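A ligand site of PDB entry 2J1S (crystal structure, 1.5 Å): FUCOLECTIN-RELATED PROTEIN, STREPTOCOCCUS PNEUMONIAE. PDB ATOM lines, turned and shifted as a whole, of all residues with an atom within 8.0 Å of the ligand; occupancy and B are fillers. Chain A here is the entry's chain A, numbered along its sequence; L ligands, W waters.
An oxygen (O3) of the ligand sits at hydrogen-bond distance from the guanidinium group (NH1) of Arg 81 (2.9 Å). NH1 of Arg 88 is in hydrogen-bond range of O3 of the ligand (2.9 Å). O3 of the ligand is in hydrogen-bond range of NE2 of His 54, at 2.7 Å.
NE of Arg 81 lies within salt-bridge range of OD2 of Asp 83 (2.9 Å). O of His 54 lies within hydrogen-bond range of N of Asp 30. NE of Arg 81 sits close to O of Ala 84, at 3.4 Å. N of Phe 47 sits at hydrogen-bond distance from OD2 of Asp 83.
Residues that only touch the ligand: Glu 85, Phe 47, Tyr 31 and Ala 84. Hydrophobic or aromatic side chains within 4 Å of the ligand: Tyr 31, Phe 47, His 54 and Ala 84. Of the 14 residues printed, 7 come within 4 Å of the ligand. The nearest printed residue that does not touch the ligand is Asp 83 (5.2 Å).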
ATOM      1  N   ASP A  30       2.713 -18.719  27.359  1.00  0.00           N
ATOM      2  CA  ASP A  30       3.003 -18.166  26.034  1.00  0.00           C
ATOM      3  C   ASP A  30       4.498 -17.831  25.962  1.00  0.00           C
ATOM      4  O   ASP A  30       5.186 -17.675  27.000  1.00  0.00           O
ATOM      5  CB  ASP A  30       2.196 -16.874  25.865  1.00  0.00           C
ATOM      6  CG  ASP A  30       1.891 -16.565  24.459  1.00  0.00           C
ATOM      7  OD1 ASP A  30       2.376 -17.272  23.536  1.00  0.00           O
ATOM      8  OD2 ASP A  30       1.143 -15.605  24.198  1.00  0.00           O
ATOM      9  N   TYR A  31       5.009 -17.748  24.727  1.00  0.00           N
ATOM     10  CA  TYR A  31       6.365 -17.345  24.464  1.00  0.00           C
ATOM     11  C   TYR A  31       7.373 -18.248  25.187  1.00  0.00           C
ATOM     12  O   TYR A  31       8.471 -17.829  25.552  1.00  0.00           O
ATOM     13  CB  TYR A  31       6.559 -15.872  24.835  1.00  0.00           C
ATOM     14  CG  TYR A  31       5.834 -14.933  23.945  1.00  0.00           C
ATOM     15  CD1 TYR A  31       4.648 -14.368  24.349  1.00  0.00           C
ATOM     16  CD2 TYR A  31       6.353 -14.567  22.727  1.00  0.00           C
ATOM     17  CE1 TYR A  31       3.972 -13.501  23.544  1.00  0.00           C
ATOM     18  CE2 TYR A  31       5.680 -13.667  21.907  1.00  0.00           C
ATOM     19  CZ  TYR A  31       4.498 -13.158  22.324  1.00  0.00           C
ATOM     20  OH  TYR A  31       3.805 -12.271  21.531  1.00  0.00           O
ATOM     21  N   PHE A  47      13.130 -10.569  29.360  1.00  0.00           N
ATOM     22  CA  PHE A  47      12.420 -11.730  28.878  1.00  0.00           C
ATOM     23  C   PHE A  47      13.268 -12.583  27.911  1.00  0.00           C
ATOM     24  O   PHE A  47      13.201 -13.806  27.932  1.00  0.00           O
ATOM     25  CB  PHE A  47      11.118 -11.370  28.151  1.00  0.00           C
ATOM     26  CG  PHE A  47      10.311 -12.563  27.871  1.00  0.00           C
ATOM     27  CD1 PHE A  47      10.263 -13.113  26.628  1.00  0.00           C
ATOM     28  CD2 PHE A  47       9.686 -13.227  28.891  1.00  0.00           C
ATOM     29  CE1 PHE A  47       9.590 -14.314  26.400  1.00  0.00           C
ATOM     30  CE2 PHE A  47       9.036 -14.403  28.654  1.00  0.00           C
ATOM     31  CZ  PHE A  47       8.989 -14.955  27.433  1.00  0.00           C
ATOM     32  N   ASN A  48      14.053 -11.913  27.092  1.00  0.00           N
ATOM     33  CA  ASN A  48      14.803 -12.613  26.055  1.00  0.00           C
ATOM     34  C   ASN A  48      15.977 -13.404  26.655  1.00  0.00           C
ATOM     35  O   ASN A  48      16.611 -14.185  25.931  1.00  0.00           O
ATOM     36  CB  ASN A  48      15.261 -11.627  24.960  1.00  0.00           C
ATOM     37  CG  ASN A  48      14.121 -11.240  23.957  1.00  0.00           C
ATOM     38  OD1 ASN A  48      12.973 -11.718  24.046  1.00  0.00           O
ATOM     39  ND2 ASN A  48      14.453 -10.376  22.989  1.00  0.00           N
ATOM     40  N   THR A  53       8.906 -15.771  33.284  1.00  0.00           N
ATOM     41  CA  THR A  53       7.689 -16.463  32.898  1.00  0.00           C
ATOM     42  C   THR A  53       6.816 -15.586  32.020  1.00  0.00           C
ATOM     43  O   THR A  53       7.034 -14.372  31.888  1.00  0.00           O
ATOM     44  CB  THR A  53       6.872 -16.890  34.153  1.00  0.00           C
ATOM     45  OG1 THR A  53       6.354 -15.718  34.816  1.00  0.00           O
ATOM     46  CG2 THR A  53       7.747 -17.633  35.203  1.00  0.00           C
ATOM     47  N   HIS A  54       5.784 -16.213  31.449  1.00  0.00           N
ATOM     48  CA  HIS A  54       4.826 -15.535  30.594  1.00  0.00           C
ATOM     49  C   HIS A  54       3.594 -16.425  30.451  1.00  0.00           C
ATOM     50  O   HIS A  54       3.690 -17.552  29.981  1.00  0.00           O
ATOM     51  CB  HIS A  54       5.457 -15.225  29.237  1.00  0.00           C
ATOM     52  CG  HIS A  54       4.873 -14.027  28.522  1.00  0.00           C
ATOM     53  ND1 HIS A  54       3.519 -13.897  28.241  1.00  0.00           N
ATOM     54  CD2 HIS A  54       5.482 -12.939  27.964  1.00  0.00           C
ATOM     55  CE1 HIS A  54       3.329 -12.790  27.538  1.00  0.00           C
ATOM     56  NE2 HIS A  54       4.496 -12.187  27.372  1.00  0.00           N
ATOM     57  N   THR A  55       2.431 -15.909  30.850  1.00  0.00           N
ATOM     58  CA  THR A  55       1.190 -16.616  30.559  1.00  0.00           C
ATOM     59  C   THR A  55       0.583 -16.004  29.289  1.00  0.00           C
ATOM     60  O   THR A  55       1.029 -14.974  28.802  1.00  0.00           O
ATOM     61  CB  THR A  55       0.157 -16.470  31.725  1.00  0.00           C
ATOM     62  OG1 THR A  55      -0.260 -15.092  31.847  1.00  0.00           O
ATOM     63  CG2 THR A  55       0.762 -16.890  33.027  1.00  0.00           C
ATOM     64  N   ARG A  81       9.455  -8.563  35.418  1.00  0.00           N
ATOM     65  CA  ARG A  81      10.024  -8.350  34.085  1.00  0.00           C
ATOM     66  C   ARG A  81      10.568  -6.885  34.064  1.00  0.00           C
ATOM     67  O   ARG A  81       9.979  -5.995  34.689  1.00  0.00           O
ATOM     68  CB  ARG A  81       8.974  -8.544  33.005  1.00  0.00           C
ATOM     69  CG  ARG A  81       9.483  -8.349  31.581  1.00  0.00           C
ATOM     70  CD  ARG A  81       8.482  -8.719  30.524  1.00  0.00           C
ATOM     71  NE  ARG A  81       9.117  -8.561  29.205  1.00  0.00           N
ATOM     72  CZ  ARG A  81       8.459  -8.727  28.056  1.00  0.00           C
ATOM     73  NH1 ARG A  81       7.159  -9.041  28.011  1.00  0.00           N
ATOM     74  NH2 ARG A  81       9.108  -8.570  26.911  1.00  0.00           N
ATOM     75  N   ASP A  83      12.517  -5.636  30.868  1.00  0.00           N
ATOM     76  CA  ASP A  83      12.863  -5.116  29.522  1.00  0.00           C
ATOM     77  C   ASP A  83      11.703  -4.394  28.834  1.00  0.00           C
ATOM     78  O   ASP A  83      11.936  -3.511  27.983  1.00  0.00           O
ATOM     79  CB  ASP A  83      13.357  -6.232  28.613  1.00  0.00           C
ATOM     80  CG  ASP A  83      12.319  -7.248  28.324  1.00  0.00           C
ATOM     81  OD1 ASP A  83      11.851  -7.422  27.168  1.00  0.00           O
ATOM     82  OD2 ASP A  83      11.922  -7.960  29.254  1.00  0.00           O
ATOM     83  N   ALA A  84      10.462  -4.744  29.173  1.00  0.00           N
ATOM     84  CA  ALA A  84       9.271  -4.190  28.501  1.00  0.00           C
ATOM     85  C   ALA A  84       8.032  -4.588  29.278  1.00  0.00           C
ATOM     86  O   ALA A  84       8.065  -5.510  30.114  1.00  0.00           O
ATOM     87  CB  ALA A  84       9.165  -4.672  27.079  1.00  0.00           C
ATOM     88  N   GLU A  85       6.951  -3.865  29.042  1.00  0.00           N
ATOM     89  CA  GLU A  85       5.623  -4.177  29.603  1.00  0.00           C
ATOM     90  C   GLU A  85       5.639  -4.353  31.091  1.00  0.00           C
ATOM     91  O   GLU A  85       4.928  -5.205  31.639  1.00  0.00           O
ATOM     92  CB  GLU A  85       5.028  -5.413  28.912  1.00  0.00           C
ATOM     93  CG  GLU A  85       4.875  -5.334  27.392  1.00  0.00           C
ATOM     94  CD  GLU A  85       4.022  -4.178  26.910  1.00  0.00           C
ATOM     95  OE1 GLU A  85       3.213  -3.613  27.695  1.00  0.00           O
ATOM     96  OE2 GLU A  85       4.145  -3.837  25.716  1.00  0.00           O
ATOM     97  N   ARG A  88       2.442  -4.502  33.543  1.00  0.00           N
ATOM     98  CA  ARG A  88       1.592  -5.671  33.674  1.00  0.00           C
ATOM     99  C   ARG A  88       1.533  -6.206  35.078  1.00  0.00           C
ATOM    100  O   ARG A  88       0.497  -6.738  35.482  1.00  0.00           O
ATOM    101  CB  ARG A  88       2.011  -6.786  32.707  1.00  0.00           C
ATOM    102  CG  ARG A  88       1.684  -6.458  31.255  1.00  0.00           C
ATOM    103  CD  ARG A  88       2.181  -7.521  30.295  1.00  0.00           C
ATOM    104  NE  ARG A  88       1.776  -7.228  28.927  1.00  0.00           N
ATOM    105  CZ  ARG A  88       2.295  -7.798  27.841  1.00  0.00           C
ATOM    106  NH1 ARG A  88       3.248  -8.712  27.942  1.00  0.00           N
ATOM    107  NH2 ARG A  88       1.861  -7.458  26.641  1.00  0.00           N
ATOM    108  N   PRO A 139      -1.311 -10.585  30.469  1.00  0.00           N
ATOM    109  CA  PRO A 139      -0.332 -11.646  30.750  1.00  0.00           C
ATOM    110  C   PRO A 139       0.429 -11.398  32.028  1.00  0.00           C
ATOM    111  O   PRO A 139       0.798 -10.262  32.359  1.00  0.00           O
ATOM    112  CB  PRO A 139       0.625 -11.591  29.565  1.00  0.00           C
ATOM    113  CG  PRO A 139      -0.129 -10.906  28.478  1.00  0.00           C
ATOM    114  CD  PRO A 139      -1.020  -9.909  29.193  1.00  0.00           C
ATOM    115  N   SER A 141       3.944 -12.058  33.857  1.00  0.00           N
ATOM    116  CA  SER A 141       5.381 -12.363  33.732  1.00  0.00           C
ATOM    117  C   SER A 141       6.138 -11.973  34.989  1.00  0.00           C
ATOM    118  O   SER A 141       6.125 -10.830  35.445  1.00  0.00           O
ATOM    119  CB  SER A 141       6.037 -11.645  32.512  1.00  0.00           C
ATOM    120  OG  SER A 141       5.543 -12.107  31.256  1.00  0.00           O
HETATM  121  C1  LIG L   1       6.804  -7.900  23.856  1.00  0.00           C
HETATM  122  C2  LIG L   1       5.334  -7.707  24.240  1.00  0.00           C
HETATM  123  O1  LIG L   1       4.799  -6.639  23.471  1.00  0.00           O
HETATM  124  C3  LIG L   1       4.561  -8.985  24.015  1.00  0.00           C
HETATM  125  O2  LIG L   1       3.234  -8.789  24.411  1.00  0.00           O
HETATM  126  C4  LIG L   1       5.201 -10.155  24.745  1.00  0.00           C
HETATM  127  O3  LIG L   1       5.142  -9.907  26.136  1.00  0.00           O
HETATM  128  C5  LIG L   1       6.679 -10.256  24.322  1.00  0.00           C
HETATM  129  C6  LIG L   1       7.442 -11.433  24.966  1.00  0.00           C
HETATM  130  O4  LIG L   1       7.305  -9.021  24.547  1.00  0.00           O
HETATM  131  O5  LIG L   1       7.532  -6.777  24.258  1.00  0.00           O
HETATM  132  O   HOH W   1       5.348  -4.142  21.620  1.00  0.00           O
